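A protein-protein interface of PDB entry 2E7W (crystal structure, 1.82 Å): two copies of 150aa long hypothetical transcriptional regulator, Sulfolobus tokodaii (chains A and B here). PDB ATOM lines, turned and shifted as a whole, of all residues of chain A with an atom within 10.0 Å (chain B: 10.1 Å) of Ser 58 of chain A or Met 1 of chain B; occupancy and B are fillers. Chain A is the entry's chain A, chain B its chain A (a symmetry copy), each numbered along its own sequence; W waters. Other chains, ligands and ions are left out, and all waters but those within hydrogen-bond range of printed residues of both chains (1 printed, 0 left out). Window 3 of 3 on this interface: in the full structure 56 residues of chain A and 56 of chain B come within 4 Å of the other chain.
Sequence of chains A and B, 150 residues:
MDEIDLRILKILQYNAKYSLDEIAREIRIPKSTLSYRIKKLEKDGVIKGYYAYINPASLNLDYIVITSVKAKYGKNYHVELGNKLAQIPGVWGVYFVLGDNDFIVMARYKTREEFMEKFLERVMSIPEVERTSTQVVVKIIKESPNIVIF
N of Asn 55 of chain A is in hydrogen-bond range of O of Val 46 of chain B (2.8 Å). O of Tyr 53 of chain A is in hydrogen-bond range of N of Lys 48 of chain B, at 2.7 Å.
The backbone carbonyl oxygen (O) of Leu 41 of chain B lies within hydrogen-bond range of the backbone NH (N) of Val 46 of chain B (2.9 Å). The backbone NH of Ile 47 of chain B lies within hydrogen-bond range of the backbone carbonyl oxygen of Leu 41 of chain B (3.2 Å). The side-chain amide nitrogen (ND2) of Asn 55 of chain A is in hydrogen-bond range of the side-chain hydroxyl (OG) of Ser 58 of chain A (2.9 Å). The backbone carbonyl oxygen (O) of Leu 59 of chain A lies close to the side-chain amino group (NZ) of Lys 110 of chain A (3.2 Å).
O of Tyr 53 of chain A touches C of Ile 47 of chain B, at 3.6 Å. O of Leu 9 of chain B touches CD1 of Ile 54 of chain A, at 3.8 Å. Val 46 of chain B touches Ile 54 of chain A (O to CA, 3.4 Å). CD1 of Ile 54 of chain A touches CG2 of Val 148 of chain B (3.6 Å). Lys 48 of chain B touches Asn 55 of chain A. Met 1 of chain B touches Ser 58 of chain A (CE to O, 3.4 Å). Leu 59 of chain A touches Leu 6 of chain B (CD2 to CD2, 3.7 Å). Leu 59 of chain A touches Val 148 of chain B. Ile 149 of chain B touches Leu 59 of chain A (CG1 to CD1, 3.99 Å). Val 148 of chain B touches Arg 108 of chain A.
Of the printed residues of chain B, Tyr 53 of chain A touches Val 46, Ile 47 and Lys 48. Of chain B, only Gly 45 (3.5 Å), Val 46 (2.8 Å) and Lys 48 (3.8 Å) come within 4 Å of Asn 55 of chain A. Met 1 of chain B touches just one residue of chain A: Ser 58 (3.4 Å). No residue of chain A comes within 4 Å of Asp 5 of chain B. Printed residues of chain A within 4 Å of Leu 9 of chain B: Ile 54. Printed residues of chain A within 4 Å of Val 46 of chain B: Tyr 53 (3.9 Å), Ile 54 (3.4 Å), Asn 55 (2.8 Å) and Ser 58 (3.6 Å). Printed residues of chain A within 4 Å of Ile 47 of chain B: Tyr 53 (3.6 Å). Printed residues of chain A within 4 Å of Ile 149 of chain B: Leu 59 (3.99 Å). The nearest printed residue of chain B that does not touch Leu 59 of chain A is Leu 9 of chain B (4.5 Å).
Of the 13 printed residues of chain A, 6 touch a printed residue of chain B. Hydrophobic or aromatic side chains of chain A that line the printed part of chain B: Tyr 53, Ile 54 and Leu 59.
No position is printed for both chains. Of the 16 pairs that touch across the chains among the printed residues, none has its exchanged pair printed and touching as well.
Water W1 lies within hydrogen-bond range of O of Val 148 of chain B and NZ of Lys 110 of chain A.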
ATOM      1  N   TYR A  53      26.379   6.508   8.147  1.00  0.00           N
ATOM      2  CA  TYR A  53      26.881   5.883   6.931  1.00  0.00           C
ATOM      3  C   TYR A  53      25.787   5.938   5.872  1.00  0.00           C
ATOM      4  O   TYR A  53      24.796   5.214   5.950  1.00  0.00           O
ATOM      5  CB  TYR A  53      27.284   4.427   7.170  1.00  0.00           C
ATOM      6  CG  TYR A  53      27.902   3.796   5.943  1.00  0.00           C
ATOM      7  CD1 TYR A  53      29.147   4.215   5.475  1.00  0.00           C
ATOM      8  CD2 TYR A  53      27.217   2.826   5.211  1.00  0.00           C
ATOM      9  CE1 TYR A  53      29.695   3.685   4.307  1.00  0.00           C
ATOM     10  CE2 TYR A  53      27.754   2.292   4.041  1.00  0.00           C
ATOM     11  CZ  TYR A  53      28.991   2.727   3.594  1.00  0.00           C
ATOM     12  OH  TYR A  53      29.523   2.208   2.433  1.00  0.00           O
ATOM     13  N   ILE A  54      25.972   6.806   4.885  1.00  0.00           N
ATOM     14  CA  ILE A  54      24.998   6.974   3.818  1.00  0.00           C
ATOM     15  C   ILE A  54      25.340   6.125   2.604  1.00  0.00           C
ATOM     16  O   ILE A  54      26.488   6.110   2.151  1.00  0.00           O
ATOM     17  CB  ILE A  54      24.920   8.450   3.382  1.00  0.00           C
ATOM     18  CG1 ILE A  54      24.553   9.318   4.585  1.00  0.00           C
ATOM     19  CG2 ILE A  54      23.902   8.615   2.257  1.00  0.00           C
ATOM     20  CD1 ILE A  54      24.781  10.797   4.366  1.00  0.00           C
ATOM     21  N   ASN A  55      24.339   5.423   2.085  1.00  0.00           N
ATOM     22  CA  ASN A  55      24.518   4.578   0.913  1.00  0.00           C
ATOM     23  C   ASN A  55      24.734   5.456  -0.318  1.00  0.00           C
ATOM     24  O   ASN A  55      23.830   6.169  -0.753  1.00  0.00           O
ATOM     25  CB  ASN A  55      23.289   3.690   0.713  1.00  0.00           C
ATOM     26  CG  ASN A  55      23.402   2.811  -0.515  1.00  0.00           C
ATOM     27  OD1 ASN A  55      24.406   2.122  -0.708  1.00  0.00           O
ATOM     28  ND2 ASN A  55      22.372   2.826  -1.352  1.00  0.00           N
ATOM     29  N   PRO A  56      25.946   5.424  -0.891  1.00  0.00           N
ATOM     30  CA  PRO A  56      26.257   6.231  -2.076  1.00  0.00           C
ATOM     31  C   PRO A  56      25.279   6.022  -3.231  1.00  0.00           C
ATOM     32  O   PRO A  56      24.964   6.958  -3.966  1.00  0.00           O
ATOM     33  CB  PRO A  56      27.679   5.796  -2.419  1.00  0.00           C
ATOM     34  CG  PRO A  56      28.262   5.500  -1.062  1.00  0.00           C
ATOM     35  CD  PRO A  56      27.147   4.714  -0.411  1.00  0.00           C
ATOM     36  N   ALA A  57      24.794   4.795  -3.385  1.00  0.00           N
ATOM     37  CA  ALA A  57      23.857   4.482  -4.457  1.00  0.00           C
ATOM     38  C   ALA A  57      22.553   5.256  -4.294  1.00  0.00           C
ATOM     39  O   ALA A  57      21.888   5.581  -5.278  1.00  0.00           O
ATOM     40  CB  ALA A  57      23.579   2.981  -4.484  1.00  0.00           C
ATOM     41  N   SER A  58      22.194   5.553  -3.046  1.00  0.00           N
ATOM     42  CA  SER A  58      20.969   6.291  -2.761  1.00  0.00           C
ATOM     43  C   SER A  58      21.085   7.731  -3.237  1.00  0.00           C
ATOM     44  O   SER A  58      20.076   8.406  -3.451  1.00  0.00           O
ATOM     45  CB  SER A  58      20.669   6.267  -1.259  1.00  0.00           C
ATOM     46  OG  SER A  58      20.482   4.941  -0.806  1.00  0.00           O
ATOM     47  N   LEU A  59      22.321   8.195  -3.397  1.00  0.00           N
ATOM     48  CA  LEU A  59      22.584   9.549  -3.864  1.00  0.00           C
ATOM     49  C   LEU A  59      22.965   9.522  -5.341  1.00  0.00           C
ATOM     50  O   LEU A  59      23.445  10.513  -5.881  1.00  0.00           O
ATOM     51  CB  LEU A  59      23.719  10.180  -3.051  1.00  0.00           C
ATOM     52  CG  LEU A  59      23.393  10.455  -1.584  1.00  0.00           C
ATOM     53  CD1 LEU A  59      24.661  10.777  -0.811  1.00  0.00           C
ATOM     54  CD2 LEU A  59      22.404  11.602  -1.512  1.00  0.00           C
ATOM     55  N   ASN A  60      22.746   8.375  -5.978  1.00  0.00           N
ATOM     56  CA  ASN A  60      23.050   8.192  -7.397  1.00  0.00           C
ATOM     57  C   ASN A  60      24.531   8.384  -7.722  1.00  0.00           C
ATOM     58  O   ASN A  60      24.873   8.825  -8.818  1.00  0.00           O
ATOM     59  CB  ASN A  60      22.212   9.158  -8.242  1.00  0.00           C
ATOM     60  CG  ASN A  60      20.726   8.845  -8.187  1.00  0.00           C
ATOM     61  OD1 ASN A  60      19.891   9.749  -8.190  1.00  0.00           O
ATOM     62  ND2 ASN A  60      20.389   7.559  -8.149  1.00  0.00           N
ATOM     63  N   LEU A  61      25.404   8.063  -6.768  1.00  0.00           N
ATOM     64  CA  LEU A  61      26.847   8.186  -6.982  1.00  0.00           C
ATOM     65  C   LEU A  61      27.277   6.922  -7.715  1.00  0.00           C
ATOM     66  O   LEU A  61      27.803   5.980  -7.117  1.00  0.00           O
ATOM     67  CB  LEU A  61      27.568   8.316  -5.639  1.00  0.00           C
ATOM     68  CG  LEU A  61      27.277   9.635  -4.914  1.00  0.00           C
ATOM     69  CD1 LEU A  61      27.861   9.607  -3.505  1.00  0.00           C
ATOM     70  CD2 LEU A  61      27.852  10.786  -5.716  1.00  0.00           C
ATOM     71  N   ASP A  62      27.048   6.933  -9.022  1.00  0.00           N
ATOM     72  CA  ASP A  62      27.320   5.797  -9.890  1.00  0.00           C
ATOM     73  C   ASP A  62      28.672   5.801 -10.600  1.00  0.00           C
ATOM     74  O   ASP A  62      29.126   4.758 -11.074  1.00  0.00           O
ATOM     75  CB  ASP A  62      26.187   5.704 -10.918  1.00  0.00           C
ATOM     76  CG  ASP A  62      26.146   4.371 -11.630  1.00  0.00           C
ATOM     77  OD1 ASP A  62      26.674   4.279 -12.758  1.00  0.00           O
ATOM     78  OD2 ASP A  62      25.590   3.412 -11.054  1.00  0.00           O
ATOM     79  N   ILE A  64      32.280   6.033  -9.941  1.00  0.00           N
ATOM     80  CA  ILE A  64      33.309   5.944  -8.906  1.00  0.00           C
ATOM     81  C   ILE A  64      34.680   5.782  -9.560  1.00  0.00           C
ATOM     82  O   ILE A  64      34.866   4.916 -10.417  1.00  0.00           O
ATOM     83  CB  ILE A  64      33.002   4.740  -7.983  1.00  0.00           C
ATOM     84  CG1 ILE A  64      31.548   4.825  -7.499  1.00  0.00           C
ATOM     85  CG2 ILE A  64      33.965   4.703  -6.809  1.00  0.00           C
ATOM     86  CD1 ILE A  64      31.194   6.103  -6.754  1.00  0.00           C
ATOM     87  N   ARG A 108      33.937  10.264  -6.000  1.00  0.00           N
ATOM     88  CA  ARG A 108      32.638   9.722  -6.384  1.00  0.00           C
ATOM     89  C   ARG A 108      31.825  10.825  -7.046  1.00  0.00           C
ATOM     90  O   ARG A 108      31.808  11.957  -6.561  1.00  0.00           O
ATOM     91  CB  ARG A 108      31.854   9.250  -5.158  1.00  0.00           C
ATOM     92  CG  ARG A 108      32.575   8.338  -4.188  1.00  0.00           C
ATOM     93  CD  ARG A 108      31.570   7.910  -3.124  1.00  0.00           C
ATOM     94  NE  ARG A 108      32.142   7.115  -2.040  1.00  0.00           N
ATOM     95  CZ  ARG A 108      32.364   7.574  -0.811  1.00  0.00           C
ATOM     96  NH1 ARG A 108      32.068   8.830  -0.500  1.00  0.00           N
ATOM     97  NH2 ARG A 108      32.869   6.768   0.113  1.00  0.00           N
ATOM     98  N   LYS A 110      28.013  11.509  -9.661  1.00  0.00           N
ATOM     99  CA  LYS A 110      26.759  10.924 -10.106  1.00  0.00           C
ATOM    100  C   LYS A 110      26.843  10.389 -11.526  1.00  0.00           C
ATOM    101  O   LYS A 110      26.266   9.348 -11.836  1.00  0.00           O
ATOM    102  CB  LYS A 110      25.635  11.959 -10.010  1.00  0.00           C
ATOM    103  CG  LYS A 110      25.251  12.300  -8.580  1.00  0.00           C
ATOM    104  CD  LYS A 110      24.172  13.369  -8.518  1.00  0.00           C
ATOM    105  CE  LYS A 110      23.588  13.455  -7.110  1.00  0.00           C
ATOM    106  NZ  LYS A 110      24.656  13.477  -6.062  1.00  0.00           N
ATOM    107  N   MET B   1      13.718  10.722  -2.039  1.00  0.00           N
ATOM    108  CA  MET B   1      13.955  11.807  -1.043  1.00  0.00           C
ATOM    109  C   MET B   1      13.945  13.179  -1.717  1.00  0.00           C
ATOM    110  O   MET B   1      14.056  13.278  -2.940  1.00  0.00           O
ATOM    111  CB  MET B   1      15.293  11.575  -0.337  1.00  0.00           C
ATOM    112  CG  MET B   1      16.500  11.564  -1.259  1.00  0.00           C
ATOM    113  SD  MET B   1      17.997  11.048  -0.395  1.00  0.00           S
ATOM    114  CE  MET B   1      18.106   9.366  -0.901  1.00  0.00           C
ATOM    115  N   ASP B   2      13.807  14.233  -0.919  1.00  0.00           N
ATOM    116  CA  ASP B   2      13.775  15.593  -1.449  1.00  0.00           C
ATOM    117  C   ASP B   2      14.933  16.450  -0.946  1.00  0.00           C
ATOM    118  O   ASP B   2      15.861  15.947  -0.310  1.00  0.00           O
ATOM    119  CB  ASP B   2      12.450  16.269  -1.087  1.00  0.00           C
ATOM    120  CG  ASP B   2      12.115  16.140   0.383  1.00  0.00           C
ATOM    121  OD1 ASP B   2      13.028  16.307   1.221  1.00  0.00           O
ATOM    122  OD2 ASP B   2      10.938  15.881   0.704  1.00  0.00           O
ATOM    123  N   GLU B   3      14.869  17.748  -1.236  1.00  0.00           N
ATOM    124  CA  GLU B   3      15.909  18.689  -0.830  1.00  0.00           C
ATOM    125  C   GLU B   3      16.088  18.731   0.686  1.00  0.00           C
ATOM    126  O   GLU B   3      17.198  18.931   1.180  1.00  0.00           O
ATOM    127  CB  GLU B   3      15.583  20.094  -1.345  1.00  0.00           C
ATOM    128  CG  GLU B   3      14.308  20.688  -0.766  1.00  0.00           C
ATOM    129  CD  GLU B   3      14.115  22.147  -1.146  1.00  0.00           C
ATOM    130  OE1 GLU B   3      14.040  22.444  -2.359  1.00  0.00           O
ATOM    131  OE2 GLU B   3      14.038  22.996  -0.230  1.00  0.00           O
ATOM    132  N   ILE B   4      14.996  18.550   1.421  1.00  0.00           N
ATOM    133  CA  ILE B   4      15.059  18.568   2.876  1.00  0.00           C
ATOM    134  C   ILE B   4      15.843  17.366   3.397  1.00  0.00           C
ATOM    135  O   ILE B   4      16.650  17.500   4.320  1.00  0.00           O
ATOM    136  CB  ILE B   4      13.642  18.597   3.498  1.00  0.00           C
ATOM    137  CG1 ILE B   4      12.973  19.937   3.164  1.00  0.00           C
ATOM    138  CG2 ILE B   4      13.723  18.422   5.016  1.00  0.00           C
ATOM    139  CD1 ILE B   4      11.570  20.092   3.712  1.00  0.00           C
ATOM    140  N   ASP B   5      15.616  16.196   2.805  1.00  0.00           N
ATOM    141  CA  ASP B   5      16.345  15.000   3.222  1.00  0.00           C
ATOM    142  C   ASP B   5      17.835  15.220   2.985  1.00  0.00           C
ATOM    143  O   ASP B   5      18.668  14.792   3.779  1.00  0.00           O
ATOM    144  CB  ASP B   5      15.899  13.770   2.428  1.00  0.00           C
ATOM    145  CG  ASP B   5      14.484  13.352   2.748  1.00  0.00           C
ATOM    146  OD1 ASP B   5      14.123  13.333   3.945  1.00  0.00           O
ATOM    147  OD2 ASP B   5      13.737  13.029   1.800  1.00  0.00           O
ATOM    148  N   LEU B   6      18.164  15.886   1.885  1.00  0.00           N
ATOM    149  CA  LEU B   6      19.560  16.152   1.561  1.00  0.00           C
ATOM    150  C   LEU B   6      20.211  17.069   2.586  1.00  0.00           C
ATOM    151  O   LEU B   6      21.383  16.903   2.913  1.00  0.00           O
ATOM    152  CB  LEU B   6      19.678  16.759   0.163  1.00  0.00           C
ATOM    153  CG  LEU B   6      19.439  15.756  -0.966  1.00  0.00           C
ATOM    154  CD1 LEU B   6      19.489  16.468  -2.309  1.00  0.00           C
ATOM    155  CD2 LEU B   6      20.500  14.662  -0.902  1.00  0.00           C
ATOM    156  N   ARG B   7      19.460  18.042   3.094  1.00  0.00           N
ATOM    157  CA  ARG B   7      20.018  18.938   4.097  1.00  0.00           C
ATOM    158  C   ARG B   7      20.249  18.168   5.393  1.00  0.00           C
ATOM    159  O   ARG B   7      21.215  18.428   6.115  1.00  0.00           O
ATOM    160  CB  ARG B   7      19.085  20.131   4.345  1.00  0.00           C
ATOM    161  CG  ARG B   7      19.043  21.115   3.184  1.00  0.00           C
ATOM    162  CD  ARG B   7      18.787  22.536   3.668  1.00  0.00           C
ATOM    163  NE  ARG B   7      17.438  22.723   4.188  1.00  0.00           N
ATOM    164  CZ  ARG B   7      16.347  22.791   3.429  1.00  0.00           C
ATOM    165  NH1 ARG B   7      16.446  22.687   2.110  1.00  0.00           N
ATOM    166  NH2 ARG B   7      15.157  22.973   3.987  1.00  0.00           N
ATOM    167  N   ILE B   8      19.364  17.215   5.680  1.00  0.00           N
ATOM    168  CA  ILE B   8      19.485  16.393   6.881  1.00  0.00           C
ATOM    169  C   ILE B   8      20.724  15.506   6.755  1.00  0.00           C
ATOM    170  O   ILE B   8      21.561  15.454   7.658  1.00  0.00           O
ATOM    171  CB  ILE B   8      18.237  15.497   7.069  1.00  0.00           C
ATOM    172  CG1 ILE B   8      17.013  16.374   7.356  1.00  0.00           C
ATOM    173  CG2 ILE B   8      18.464  14.501   8.196  1.00  0.00           C
ATOM    174  CD1 ILE B   8      15.711  15.610   7.374  1.00  0.00           C
ATOM    175  N   LEU B   9      20.839  14.812   5.628  1.00  0.00           N
ATOM    176  CA  LEU B   9      21.981  13.932   5.398  1.00  0.00           C
ATOM    177  C   LEU B   9      23.299  14.706   5.411  1.00  0.00           C
ATOM    178  O   LEU B   9      24.317  14.206   5.900  1.00  0.00           O
ATOM    179  CB  LEU B   9      21.816  13.188   4.062  1.00  0.00           C
ATOM    180  CG  LEU B   9      20.637  12.203   3.969  1.00  0.00           C
ATOM    181  CD1 LEU B   9      20.489  11.706   2.534  1.00  0.00           C
ATOM    182  CD2 LEU B   9      20.859  11.029   4.925  1.00  0.00           C
ATOM    183  N   LYS B  10      23.288  15.929   4.889  1.00  0.00           N
ATOM    184  CA  LYS B  10      24.512  16.722   4.860  1.00  0.00           C
ATOM    185  C   LYS B  10      25.030  16.963   6.275  1.00  0.00           C
ATOM    186  O   LYS B  10      26.238  17.076   6.493  1.00  0.00           O
ATOM    187  CB  LYS B  10      24.282  18.054   4.141  1.00  0.00           C
ATOM    188  CG  LYS B  10      25.575  18.800   3.848  1.00  0.00           C
ATOM    189  CD  LYS B  10      25.344  20.018   2.968  1.00  0.00           C
ATOM    190  CE  LYS B  10      26.660  20.717   2.659  1.00  0.00           C
ATOM    191  NZ  LYS B  10      26.457  21.923   1.811  1.00  0.00           N
ATOM    192  N   ARG B  37      11.369  11.833   9.067  1.00  0.00           N
ATOM    193  CA  ARG B  37      12.204  11.769   7.875  1.00  0.00           C
ATOM    194  C   ARG B  37      13.444  10.911   8.100  1.00  0.00           C
ATOM    195  O   ARG B  37      13.842  10.151   7.220  1.00  0.00           O
ATOM    196  CB  ARG B  37      12.612  13.177   7.443  1.00  0.00           C
ATOM    197  CG  ARG B  37      11.513  13.941   6.717  1.00  0.00           C
ATOM    198  CD  ARG B  37      11.863  15.412   6.599  1.00  0.00           C
ATOM    199  NE  ARG B  37      11.003  16.116   5.651  1.00  0.00           N
ATOM    200  CZ  ARG B  37      11.134  16.050   4.329  1.00  0.00           C
ATOM    201  NH1 ARG B  37      12.093  15.312   3.787  1.00  0.00           N
ATOM    202  NH2 ARG B  37      10.306  16.731   3.545  1.00  0.00           N
ATOM    203  N   ILE B  38      14.057  11.032   9.273  1.00  0.00           N
ATOM    204  CA  ILE B  38      15.248  10.242   9.571  1.00  0.00           C
ATOM    205  C   ILE B  38      14.879   8.763   9.656  1.00  0.00           C
ATOM    206  O   ILE B  38      15.583   7.910   9.117  1.00  0.00           O
ATOM    207  CB  ILE B  38      15.913  10.700  10.888  1.00  0.00           C
ATOM    208  CG1 ILE B  38      16.525  12.091  10.692  1.00  0.00           C
ATOM    209  CG2 ILE B  38      16.986   9.705  11.313  1.00  0.00           C
ATOM    210  CD1 ILE B  38      17.086  12.709  11.956  1.00  0.00           C
ATOM    211  N   LYS B  40      12.531   7.251   8.153  1.00  0.00           N
ATOM    212  CA  LYS B  40      12.240   6.751   6.815  1.00  0.00           C
ATOM    213  C   LYS B  40      13.519   6.521   6.016  1.00  0.00           C
ATOM    214  O   LYS B  40      13.625   5.540   5.282  1.00  0.00           O
ATOM    215  CB  LYS B  40      11.326   7.718   6.058  1.00  0.00           C
ATOM    216  CG  LYS B  40      11.054   7.281   4.627  1.00  0.00           C
ATOM    217  CD  LYS B  40       9.984   8.124   3.958  1.00  0.00           C
ATOM    218  CE  LYS B  40       9.772   7.669   2.523  1.00  0.00           C
ATOM    219  NZ  LYS B  40       9.531   6.198   2.451  1.00  0.00           N
ATOM    220  N   LEU B  41      14.487   7.422   6.155  1.00  0.00           N
ATOM    221  CA  LEU B  41      15.754   7.276   5.444  1.00  0.00           C
ATOM    222  C   LEU B  41      16.455   5.998   5.892  1.00  0.00           C
ATOM    223  O   LEU B  41      17.127   5.342   5.102  1.00  0.00           O
ATOM    224  CB  LEU B  41      16.661   8.485   5.707  1.00  0.00           C
ATOM    225  CG  LEU B  41      16.191   9.811   5.107  1.00  0.00           C
ATOM    226  CD1 LEU B  41      17.006  10.963   5.683  1.00  0.00           C
ATOM    227  CD2 LEU B  41      16.315   9.756   3.594  1.00  0.00           C
ATOM    228  N   GLU B  42      16.298   5.647   7.166  1.00  0.00           N
ATOM    229  CA  GLU B  42      16.916   4.435   7.694  1.00  0.00           C
ATOM    230  C   GLU B  42      16.169   3.221   7.149  1.00  0.00           C
ATOM    231  O   GLU B  42      16.782   2.246   6.710  1.00  0.00           O
ATOM    232  CB  GLU B  42      16.875   4.437   9.226  1.00  0.00           C
ATOM    233  CG  GLU B  42      17.507   5.675   9.858  1.00  0.00           C
ATOM    234  CD  GLU B  42      17.399   5.688  11.372  1.00  0.00           C
ATOM    235  OE1 GLU B  42      16.401   5.157  11.907  1.00  0.00           O
ATOM    236  OE2 GLU B  42      18.302   6.244  12.030  1.00  0.00           O
ATOM    237  N   LYS B  43      14.841   3.293   7.165  1.00  0.00           N
ATOM    238  CA  LYS B  43      14.005   2.204   6.667  1.00  0.00           C
ATOM    239  C   LYS B  43      14.208   1.949   5.177  1.00  0.00           C
ATOM    240  O   LYS B  43      14.136   0.807   4.724  1.00  0.00           O
ATOM    241  CB  LYS B  43      12.525   2.507   6.924  1.00  0.00           C
ATOM    242  CG  LYS B  43      12.111   2.436   8.385  1.00  0.00           C
ATOM    243  CD  LYS B  43      12.216   1.017   8.927  1.00  0.00           C
ATOM    244  CE  LYS B  43      11.731   0.940  10.368  1.00  0.00           C
ATOM    245  NZ  LYS B  43      10.303   1.349  10.500  1.00  0.00           N
ATOM    246  N   ASP B  44      14.459   3.010   4.417  1.00  0.00           N
ATOM    247  CA  ASP B  44      14.654   2.881   2.976  1.00  0.00           C
ATOM    248  C   ASP B  44      16.081   2.520   2.577  1.00  0.00           C
ATOM    249  O   ASP B  44      16.392   2.432   1.391  1.00  0.00           O
ATOM    250  CB  ASP B  44      14.231   4.173   2.272  1.00  0.00           C
ATOM    251  CG  ASP B  44      12.737   4.413   2.352  1.00  0.00           C
ATOM    252  OD1 ASP B  44      12.046   3.621   3.027  1.00  0.00           O
ATOM    253  OD2 ASP B  44      12.253   5.392   1.743  1.00  0.00           O
ATOM    254  N   GLY B  45      16.945   2.316   3.564  1.00  0.00           N
ATOM    255  CA  GLY B  45      18.319   1.951   3.272  1.00  0.00           C
ATOM    256  C   GLY B  45      19.232   3.085   2.840  1.00  0.00           C
ATOM    257  O   GLY B  45      20.340   2.830   2.366  1.00  0.00           O
ATOM    258  N   VAL B  46      18.781   4.329   2.984  1.00  0.00           N
ATOM    259  CA  VAL B  46      19.606   5.480   2.614  1.00  0.00           C
ATOM    260  C   VAL B  46      20.686   5.626   3.683  1.00  0.00           C
ATOM    261  O   VAL B  46      21.873   5.758   3.373  1.00  0.00           O
ATOM    262  CB  VAL B  46      18.763   6.769   2.526  1.00  0.00           C
ATOM    263  CG1 VAL B  46      19.657   7.969   2.218  1.00  0.00           C
ATOM    264  CG2 VAL B  46      17.706   6.608   1.442  1.00  0.00           C
ATOM    265  N   ILE B  47      20.266   5.611   4.946  1.00  0.00           N
ATOM    266  CA  ILE B  47      21.193   5.672   6.066  1.00  0.00           C
ATOM    267  C   ILE B  47      21.384   4.207   6.451  1.00  0.00           C
ATOM    268  O   ILE B  47      20.465   3.574   6.969  1.00  0.00           O
ATOM    269  CB  ILE B  47      20.604   6.446   7.270  1.00  0.00           C
ATOM    270  CG1 ILE B  47      20.464   7.927   6.917  1.00  0.00           C
ATOM    271  CG2 ILE B  47      21.497   6.261   8.489  1.00  0.00           C
ATOM    272  CD1 ILE B  47      19.768   8.761   7.983  1.00  0.00           C
ATOM    273  N   LYS B  48      22.575   3.678   6.177  1.00  0.00           N
ATOM    274  CA  LYS B  48      22.907   2.279   6.445  1.00  0.00           C
ATOM    275  C   LYS B  48      23.246   1.975   7.897  1.00  0.00           C
ATOM    276  O   LYS B  48      23.136   0.831   8.345  1.00  0.00           O
ATOM    277  CB  LYS B  48      24.088   1.860   5.568  1.00  0.00           C
ATOM    278  CG  LYS B  48      23.855   2.043   4.078  1.00  0.00           C
ATOM    279  CD  LYS B  48      23.143   0.848   3.476  1.00  0.00           C
ATOM    280  CE  LYS B  48      24.024  -0.392   3.544  1.00  0.00           C
ATOM    281  NZ  LYS B  48      23.390  -1.563   2.883  1.00  0.00           N
ATOM    282  N   VAL B 148      29.684  12.342   1.555  1.00  0.00           N
ATOM    283  CA  VAL B 148      29.063  11.986   0.291  1.00  0.00           C
ATOM    284  C   VAL B 148      28.357  13.182  -0.340  1.00  0.00           C
ATOM    285  O   VAL B 148      28.063  13.179  -1.533  1.00  0.00           O
ATOM    286  CB  VAL B 148      28.058  10.832   0.483  1.00  0.00           C
ATOM    287  CG1 VAL B 148      28.812   9.528   0.739  1.00  0.00           C
ATOM    288  CG2 VAL B 148      27.134  11.129   1.656  1.00  0.00           C
ATOM    289  N   ILE B 149      28.095  14.203   0.471  1.00  0.00           N
ATOM    290  CA  ILE B 149      27.430  15.422   0.008  1.00  0.00           C
ATOM    291  C   ILE B 149      28.377  16.602   0.219  1.00  0.00           C
ATOM    292  O   ILE B 149      28.674  16.976   1.355  1.00  0.00           O
ATOM    293  CB  ILE B 149      26.119  15.660   0.796  1.00  0.00           C
ATOM    294  CG1 ILE B 149      25.166  14.484   0.571  1.00  0.00           C
ATOM    295  CG2 ILE B 149      25.464  16.968   0.355  1.00  0.00           C
ATOM    296  CD1 ILE B 149      23.939  14.502   1.460  1.00  0.00           C
HETATM  297  O   HOH W   1      26.323  14.248  -3.399  1.00  0.00           O
